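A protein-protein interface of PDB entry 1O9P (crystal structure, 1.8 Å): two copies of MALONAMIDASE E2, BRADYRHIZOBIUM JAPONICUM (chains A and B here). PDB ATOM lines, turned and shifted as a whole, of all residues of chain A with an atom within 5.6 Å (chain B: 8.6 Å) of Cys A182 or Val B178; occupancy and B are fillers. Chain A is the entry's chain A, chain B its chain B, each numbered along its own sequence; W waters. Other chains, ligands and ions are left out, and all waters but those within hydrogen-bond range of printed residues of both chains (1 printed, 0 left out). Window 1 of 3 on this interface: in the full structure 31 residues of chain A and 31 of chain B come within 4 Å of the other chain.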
ATOM      1  N   VAL A 180     -23.441  18.577  31.118  1.00  0.00           N
ATOM      2  CA  VAL A 180     -22.480  19.668  31.267  1.00  0.00           C
ATOM      3  C   VAL A 180     -21.605  19.642  30.009  1.00  0.00           C
ATOM      4  O   VAL A 180     -20.910  18.655  29.761  1.00  0.00           O
ATOM      5  CB  VAL A 180     -21.591  19.457  32.520  1.00  0.00           C
ATOM      6  CG1 VAL A 180     -20.583  20.580  32.655  1.00  0.00           C
ATOM      7  CG2 VAL A 180     -22.465  19.371  33.768  1.00  0.00           C
ATOM      8  N   LYS A 181     -21.659  20.711  29.212  1.00  0.00           N
ATOM      9  CA  LYS A 181     -20.884  20.796  27.970  1.00  0.00           C
ATOM     10  C   LYS A 181     -19.440  20.394  28.238  1.00  0.00           C
ATOM     11  O   LYS A 181     -18.769  20.988  29.080  1.00  0.00           O
ATOM     12  CB  LYS A 181     -20.931  22.224  27.415  1.00  0.00           C
ATOM     13  CG  LYS A 181     -20.302  22.392  26.040  1.00  0.00           C
ATOM     14  CD  LYS A 181     -21.032  21.584  24.990  1.00  0.00           C
ATOM     15  CE  LYS A 181     -20.463  21.853  23.602  1.00  0.00           C
ATOM     16  NZ  LYS A 181     -20.897  20.816  22.636  1.00  0.00           N
ATOM     17  N   CYS A 182     -18.957  19.393  27.514  1.00  0.00           N
ATOM     18  CA  CYS A 182     -17.601  18.911  27.732  1.00  0.00           C
ATOM     19  C   CYS A 182     -16.501  19.716  27.051  1.00  0.00           C
ATOM     20  O   CYS A 182     -16.647  20.173  25.917  1.00  0.00           O
ATOM     21  CB  CYS A 182     -17.495  17.445  27.302  1.00  0.00           C
ATOM     22  SG  CYS A 182     -15.871  16.703  27.642  1.00  0.00           S
ATOM     23  N   TYR A 183     -15.404  19.900  27.777  1.00  0.00           N
ATOM     24  CA  TYR A 183     -14.226  20.602  27.273  1.00  0.00           C
ATOM     25  C   TYR A 183     -13.186  19.478  27.227  1.00  0.00           C
ATOM     26  O   TYR A 183     -12.650  19.148  26.166  1.00  0.00           O
ATOM     27  CB  TYR A 183     -13.819  21.707  28.258  1.00  0.00           C
ATOM     28  CG  TYR A 183     -12.698  22.635  27.812  1.00  0.00           C
ATOM     29  CD1 TYR A 183     -12.371  23.756  28.573  1.00  0.00           C
ATOM     30  CD2 TYR A 183     -11.971  22.403  26.642  1.00  0.00           C
ATOM     31  CE1 TYR A 183     -11.357  24.625  28.192  1.00  0.00           C
ATOM     32  CE2 TYR A 183     -10.943  23.275  26.247  1.00  0.00           C
ATOM     33  CZ  TYR A 183     -10.649  24.385  27.032  1.00  0.00           C
ATOM     34  OH  TYR A 183      -9.659  25.267  26.668  1.00  0.00           O
ATOM     35  N   SER A 184     -12.939  18.877  28.389  1.00  0.00           N
ATOM     36  CA  SER A 184     -12.015  17.755  28.524  1.00  0.00           C
ATOM     37  C   SER A 184     -12.603  16.783  29.546  1.00  0.00           C
ATOM     38  O   SER A 184     -12.660  17.086  30.739  1.00  0.00           O
ATOM     39  CB  SER A 184     -10.642  18.235  28.999  1.00  0.00           C
ATOM     40  OG  SER A 184      -9.819  17.128  29.334  1.00  0.00           O
ATOM     41  N   TRP A 185     -13.044  15.615  29.088  1.00  0.00           N
ATOM     42  CA  TRP A 185     -13.645  14.641  29.999  1.00  0.00           C
ATOM     43  C   TRP A 185     -12.705  14.121  31.085  1.00  0.00           C
ATOM     44  O   TRP A 185     -13.153  13.664  32.136  1.00  0.00           O
ATOM     45  CB  TRP A 185     -14.265  13.477  29.207  1.00  0.00           C
ATOM     46  CG  TRP A 185     -13.310  12.682  28.359  1.00  0.00           C
ATOM     47  CD1 TRP A 185     -12.549  11.615  28.754  1.00  0.00           C
ATOM     48  CD2 TRP A 185     -13.031  12.880  26.966  1.00  0.00           C
ATOM     49  NE1 TRP A 185     -11.818  11.132  27.688  1.00  0.00           N
ATOM     50  CE2 TRP A 185     -12.095  11.892  26.581  1.00  0.00           C
ATOM     51  CE3 TRP A 185     -13.481  13.797  26.005  1.00  0.00           C
ATOM     52  CZ2 TRP A 185     -11.600  11.794  25.276  1.00  0.00           C
ATOM     53  CZ3 TRP A 185     -12.988  13.698  24.705  1.00  0.00           C
ATOM     54  CH2 TRP A 185     -12.057  12.704  24.355  1.00  0.00           C
ATOM     55  N   ASP A 188     -12.869  18.052  33.303  1.00  0.00           N
ATOM     56  CA  ASP A 188     -14.100  18.726  33.714  1.00  0.00           C
ATOM     57  C   ASP A 188     -14.611  18.265  35.072  1.00  0.00           C
ATOM     58  O   ASP A 188     -14.870  17.084  35.278  1.00  0.00           O
ATOM     59  CB  ASP A 188     -15.207  18.520  32.670  1.00  0.00           C
ATOM     60  CG  ASP A 188     -14.897  19.182  31.335  1.00  0.00           C
ATOM     61  OD1 ASP A 188     -13.809  19.785  31.190  1.00  0.00           O
ATOM     62  OD2 ASP A 188     -15.746  19.090  30.423  1.00  0.00           O
ATOM     63  N   ALA A 284     -13.982  16.481  21.865  1.00  0.00           N
ATOM     64  CA  ALA A 284     -15.198  16.969  22.521  1.00  0.00           C
ATOM     65  C   ALA A 284     -15.918  18.086  21.777  1.00  0.00           C
ATOM     66  O   ALA A 284     -17.138  18.209  21.870  1.00  0.00           O
ATOM     67  CB  ALA A 284     -14.876  17.427  23.937  1.00  0.00           C
ATOM     68  N   LEU A 285     -15.162  18.896  21.048  1.00  0.00           N
ATOM     69  CA  LEU A 285     -15.740  20.005  20.300  1.00  0.00           C
ATOM     70  C   LEU A 285     -15.550  19.766  18.804  1.00  0.00           C
ATOM     71  O   LEU A 285     -15.493  20.710  18.014  1.00  0.00           O
ATOM     72  CB  LEU A 285     -15.066  21.319  20.719  1.00  0.00           C
ATOM     73  CG  LEU A 285     -15.221  21.698  22.196  1.00  0.00           C
ATOM     74  CD1 LEU A 285     -14.347  22.898  22.527  1.00  0.00           C
ATOM     75  CD2 LEU A 285     -16.683  21.994  22.496  1.00  0.00           C
ATOM     76  N   ILE B  64     -29.080   6.602  21.187  1.00  0.00           N
ATOM     77  CA  ILE B  64     -28.876   7.326  22.436  1.00  0.00           C
ATOM     78  C   ILE B  64     -27.630   8.161  22.159  1.00  0.00           C
ATOM     79  O   ILE B  64     -27.128   8.867  23.029  1.00  0.00           O
ATOM     80  CB  ILE B  64     -28.613   6.427  23.680  1.00  0.00           C
ATOM     81  CG1 ILE B  64     -27.552   5.373  23.378  1.00  0.00           C
ATOM     82  CG2 ILE B  64     -29.924   5.814  24.159  1.00  0.00           C
ATOM     83  CD1 ILE B  64     -26.995   4.715  24.637  1.00  0.00           C
ATOM     84  N   ILE B  65     -27.141   8.066  20.924  1.00  0.00           N
ATOM     85  CA  ILE B  65     -25.959   8.804  20.497  1.00  0.00           C
ATOM     86  C   ILE B  65     -26.386   9.990  19.634  1.00  0.00           C
ATOM     87  O   ILE B  65     -27.026   9.825  18.594  1.00  0.00           O
ATOM     88  CB  ILE B  65     -24.995   7.895  19.700  1.00  0.00           C
ATOM     89  CG1 ILE B  65     -24.624   6.676  20.561  1.00  0.00           C
ATOM     90  CG2 ILE B  65     -23.726   8.672  19.325  1.00  0.00           C
ATOM     91  CD1 ILE B  65     -23.768   5.635  19.858  1.00  0.00           C
ATOM     92  N   ASP B  66     -26.018  11.187  20.078  1.00  0.00           N
ATOM     93  CA  ASP B  66     -26.373  12.425  19.388  1.00  0.00           C
ATOM     94  C   ASP B  66     -25.969  12.562  17.923  1.00  0.00           C
ATOM     95  O   ASP B  66     -24.836  12.273  17.547  1.00  0.00           O
ATOM     96  CB  ASP B  66     -25.777  13.641  20.112  1.00  0.00           C
ATOM     97  CG  ASP B  66     -26.448  13.941  21.437  1.00  0.00           C
ATOM     98  OD1 ASP B  66     -27.510  13.358  21.738  1.00  0.00           O
ATOM     99  OD2 ASP B  66     -25.898  14.789  22.173  1.00  0.00           O
ATOM    100  N   SER B  86     -25.662  19.133  18.199  1.00  0.00           N
ATOM    101  CA  SER B  86     -24.411  18.616  17.653  1.00  0.00           C
ATOM    102  C   SER B  86     -24.311  17.105  17.498  1.00  0.00           C
ATOM    103  O   SER B  86     -25.046  16.346  18.129  1.00  0.00           O
ATOM    104  CB  SER B  86     -23.252  19.071  18.538  1.00  0.00           C
ATOM    105  OG  SER B  86     -23.409  18.566  19.856  1.00  0.00           O
ATOM    106  N   ASP B  87     -23.387  16.685  16.640  1.00  0.00           N
ATOM    107  CA  ASP B  87     -23.109  15.272  16.430  1.00  0.00           C
ATOM    108  C   ASP B  87     -22.181  14.909  17.583  1.00  0.00           C
ATOM    109  O   ASP B  87     -21.293  15.693  17.931  1.00  0.00           O
ATOM    110  CB  ASP B  87     -22.362  15.047  15.110  1.00  0.00           C
ATOM    111  CG  ASP B  87     -23.262  15.163  13.895  1.00  0.00           C
ATOM    112  OD1 ASP B  87     -24.324  14.506  13.877  1.00  0.00           O
ATOM    113  OD2 ASP B  87     -22.901  15.901  12.954  1.00  0.00           O
ATOM    114  N   ALA B  88     -22.377  13.739  18.180  1.00  0.00           N
ATOM    115  CA  ALA B  88     -21.517  13.307  19.279  1.00  0.00           C
ATOM    116  C   ALA B  88     -20.089  13.139  18.760  1.00  0.00           C
ATOM    117  O   ALA B  88     -19.880  12.820  17.592  1.00  0.00           O
ATOM    118  CB  ALA B  88     -22.016  11.981  19.847  1.00  0.00           C
ATOM    119  N   PRO B  89     -19.086  13.349  19.625  1.00  0.00           N
ATOM    120  CA  PRO B  89     -17.702  13.195  19.176  1.00  0.00           C
ATOM    121  C   PRO B  89     -17.439  11.890  18.411  1.00  0.00           C
ATOM    122  O   PRO B  89     -16.774  11.912  17.381  1.00  0.00           O
ATOM    123  CB  PRO B  89     -16.913  13.291  20.474  1.00  0.00           C
ATOM    124  CG  PRO B  89     -17.695  14.320  21.238  1.00  0.00           C
ATOM    125  CD  PRO B  89     -19.138  13.896  20.995  1.00  0.00           C
ATOM    126  N   VAL B  90     -17.967  10.761  18.889  1.00  0.00           N
ATOM    127  CA  VAL B  90     -17.736   9.499  18.183  1.00  0.00           C
ATOM    128  C   VAL B  90     -18.334   9.504  16.779  1.00  0.00           C
ATOM    129  O   VAL B  90     -17.806   8.862  15.873  1.00  0.00           O
ATOM    130  CB  VAL B  90     -18.256   8.267  18.972  1.00  0.00           C
ATOM    131  CG1 VAL B  90     -17.473   8.129  20.257  1.00  0.00           C
ATOM    132  CG2 VAL B  90     -19.747   8.386  19.261  1.00  0.00           C
ATOM    133  N   VAL B  91     -19.431  10.232  16.597  1.00  0.00           N
ATOM    134  CA  VAL B  91     -20.045  10.347  15.280  1.00  0.00           C
ATOM    135  C   VAL B  91     -19.112  11.192  14.410  1.00  0.00           C
ATOM    136  O   VAL B  91     -18.905  10.897  13.235  1.00  0.00           O
ATOM    137  CB  VAL B  91     -21.428  11.028  15.361  1.00  0.00           C
ATOM    138  CG1 VAL B  91     -21.945  11.332  13.961  1.00  0.00           C
ATOM    139  CG2 VAL B  91     -22.406  10.122  16.113  1.00  0.00           C
ATOM    140  N   MET B  92     -18.545  12.244  14.994  1.00  0.00           N
ATOM    141  CA  MET B  92     -17.621  13.105  14.261  1.00  0.00           C
ATOM    142  C   MET B  92     -16.357  12.336  13.887  1.00  0.00           C
ATOM    143  O   MET B  92     -15.746  12.609  12.856  1.00  0.00           O
ATOM    144  CB  MET B  92     -17.241  14.339  15.091  1.00  0.00           C
ATOM    145  CG  MET B  92     -18.347  15.382  15.213  1.00  0.00           C
ATOM    146  SD  MET B  92     -18.974  15.920  13.591  1.00  0.00           S
ATOM    147  CE  MET B  92     -17.463  16.480  12.819  1.00  0.00           C
ATOM    148  N   LEU B 175     -12.966   5.568  23.686  1.00  0.00           N
ATOM    149  CA  LEU B 175     -13.873   6.340  22.847  1.00  0.00           C
ATOM    150  C   LEU B 175     -14.686   7.218  23.797  1.00  0.00           C
ATOM    151  O   LEU B 175     -15.177   6.750  24.827  1.00  0.00           O
ATOM    152  CB  LEU B 175     -14.797   5.411  22.053  1.00  0.00           C
ATOM    153  CG  LEU B 175     -14.129   4.435  21.071  1.00  0.00           C
ATOM    154  CD1 LEU B 175     -15.197   3.589  20.395  1.00  0.00           C
ATOM    155  CD2 LEU B 175     -13.324   5.201  20.030  1.00  0.00           C
ATOM    156  N   PRO B 176     -14.829   8.510  23.471  1.00  0.00           N
ATOM    157  CA  PRO B 176     -15.586   9.427  24.324  1.00  0.00           C
ATOM    158  C   PRO B 176     -17.080   9.135  24.387  1.00  0.00           C
ATOM    159  O   PRO B 176     -17.688   8.713  23.400  1.00  0.00           O
ATOM    160  CB  PRO B 176     -15.285  10.791  23.706  1.00  0.00           C
ATOM    161  CG  PRO B 176     -15.140  10.472  22.263  1.00  0.00           C
ATOM    162  CD  PRO B 176     -14.297   9.213  22.291  1.00  0.00           C
ATOM    163  N   THR B 177     -17.662   9.371  25.557  1.00  0.00           N
ATOM    164  CA  THR B 177     -19.086   9.153  25.760  1.00  0.00           C
ATOM    165  C   THR B 177     -19.831  10.487  25.735  1.00  0.00           C
ATOM    166  O   THR B 177     -20.993  10.579  26.125  1.00  0.00           O
ATOM    167  CB  THR B 177     -19.342   8.425  27.092  1.00  0.00           C
ATOM    168  OG1 THR B 177     -18.580   9.047  28.131  1.00  0.00           O
ATOM    169  CG2 THR B 177     -18.931   6.965  26.979  1.00  0.00           C
ATOM    170  N   VAL B 178     -19.143  11.530  25.282  1.00  0.00           N
ATOM    171  CA  VAL B 178     -19.766  12.842  25.172  1.00  0.00           C
ATOM    172  C   VAL B 178     -20.864  12.688  24.120  1.00  0.00           C
ATOM    173  O   VAL B 178     -20.651  12.049  23.095  1.00  0.00           O
ATOM    174  CB  VAL B 178     -18.744  13.899  24.699  1.00  0.00           C
ATOM    175  CG1 VAL B 178     -19.445  15.225  24.415  1.00  0.00           C
ATOM    176  CG2 VAL B 178     -17.668  14.087  25.770  1.00  0.00           C
ATOM    177  N   GLY B 179     -22.038  13.253  24.387  1.00  0.00           N
ATOM    178  CA  GLY B 179     -23.128  13.154  23.434  1.00  0.00           C
ATOM    179  C   GLY B 179     -23.759  11.776  23.415  1.00  0.00           C
ATOM    180  O   GLY B 179     -24.433  11.404  22.454  1.00  0.00           O
ATOM    181  N   VAL B 180     -23.526  11.008  24.473  1.00  0.00           N
ATOM    182  CA  VAL B 180     -24.094   9.671  24.594  1.00  0.00           C
ATOM    183  C   VAL B 180     -24.935   9.675  25.865  1.00  0.00           C
ATOM    184  O   VAL B 180     -24.396   9.827  26.960  1.00  0.00           O
ATOM    185  CB  VAL B 180     -22.992   8.596  24.726  1.00  0.00           C
ATOM    186  CG1 VAL B 180     -23.624   7.219  24.867  1.00  0.00           C
ATOM    187  CG2 VAL B 180     -22.073   8.642  23.518  1.00  0.00           C
ATOM    188  N   LYS B 181     -26.249   9.526  25.713  1.00  0.00           N
ATOM    189  CA  LYS B 181     -27.167   9.527  26.850  1.00  0.00           C
ATOM    190  C   LYS B 181     -26.621   8.648  27.962  1.00  0.00           C
ATOM    191  O   LYS B 181     -26.450   7.440  27.790  1.00  0.00           O
ATOM    192  CB  LYS B 181     -28.548   9.030  26.415  1.00  0.00           C
ATOM    193  CG  LYS B 181     -29.628   9.127  27.491  1.00  0.00           C
ATOM    194  CD  LYS B 181     -29.816  10.551  27.978  1.00  0.00           C
ATOM    195  CE  LYS B 181     -31.032  10.664  28.897  1.00  0.00           C
ATOM    196  NZ  LYS B 181     -31.003  11.922  29.685  1.00  0.00           N
ATOM    197  N   CYS B 182     -26.353   9.255  29.111  1.00  0.00           N
ATOM    198  CA  CYS B 182     -25.785   8.516  30.231  1.00  0.00           C
ATOM    199  C   CYS B 182     -26.742   7.615  31.004  1.00  0.00           C
ATOM    200  O   CYS B 182     -27.872   7.997  31.313  1.00  0.00           O
ATOM    201  CB  CYS B 182     -25.115   9.489  31.209  1.00  0.00           C
ATOM    202  SG  CYS B 182     -24.282   8.672  32.607  1.00  0.00           S
ATOM    203  N   ASP B 188     -20.795   3.173  31.189  1.00  0.00           N
ATOM    204  CA  ASP B 188     -21.056   3.432  29.774  1.00  0.00           C
ATOM    205  C   ASP B 188     -19.799   3.404  28.910  1.00  0.00           C
ATOM    206  O   ASP B 188     -18.845   4.141  29.153  1.00  0.00           O
ATOM    207  CB  ASP B 188     -21.772   4.780  29.601  1.00  0.00           C
ATOM    208  CG  ASP B 188     -23.188   4.776  30.175  1.00  0.00           C
ATOM    209  OD1 ASP B 188     -23.591   3.779  30.818  1.00  0.00           O
ATOM    210  OD2 ASP B 188     -23.902   5.786  29.987  1.00  0.00           O
ATOM    211  N   VAL B 190     -18.681   3.018  24.624  1.00  0.00           N
ATOM    212  CA  VAL B 190     -19.091   2.906  23.229  1.00  0.00           C
ATOM    213  C   VAL B 190     -18.498   1.624  22.644  1.00  0.00           C
ATOM    214  O   VAL B 190     -17.412   1.200  23.045  1.00  0.00           O
ATOM    215  CB  VAL B 190     -18.586   4.104  22.394  1.00  0.00           C
ATOM    216  CG1 VAL B 190     -19.019   3.946  20.940  1.00  0.00           C
ATOM    217  CG2 VAL B 190     -19.125   5.403  22.975  1.00  0.00           C
HETATM  218  O   HOH W   1     -13.889   8.871  27.043  1.00  0.00           O
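Of the printed residues of chain B, Trp A185 touches Pro B176 (3.8 Å). Of the printed residues of chain B, Ala A284 touches Pro B89 (3.9 Å). Asp B87 touches none of the printed residues of chain A. Of the printed residues of chain A, Pro B89 touches Ala A284. Leu B175 touches none of the printed residues of chain A. Of the printed residues of chain A, Pro B176 touches Trp A185 (3.8 Å). Val B178 touches just one residue of chain A: Cys A182.
4 positions are printed for both chains. Of the 3 pairs that touch across the chains among the printed residues, none has its exchanged pair printed and touching as well.
Water W1 lies within hydrogen-bond range of the indole nitrogen of Trp A185 (3.1 Å) and the backbone carbonyl oxygen of Leu B175 (3.3 Å).
Cys A182 touches Val B178 (SG to CG2, 3.7 Å). Trp A185 touches Pro B176 (CH2 to CB, 3.8 Å). Ala A284 touches Pro B89.
Of the 20 printed residues of chain B, 3 touch a printed residue of chain A. Hydrophobic or aromatic side chains of chain B that line the printed part of chain A: Pro B89, Pro B176 and Val B178. Of the 9 printed residues of chain A, 3 touch a printed residue of chain B. Printed residues of chain A that touch a printed residue of chain B: Cys A182, Trp A185 and Ala A284. Among the printed residues, no Asp or Glu carboxylate lies within 4 Å of a Lys or Arg side-chain nitrogen of the other chain.
SG of Cys A182 is in hydrogen-bond range of N of Ser A184 (3.7 Å). N of Trp A185 sits at hydrogen-bond distance from SG of Cys A182. The side-chain sulfur (SG) of Cys A182 lies close to the side-chain carboxylate (OD2) of Asp A188, 3.7 Å away.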
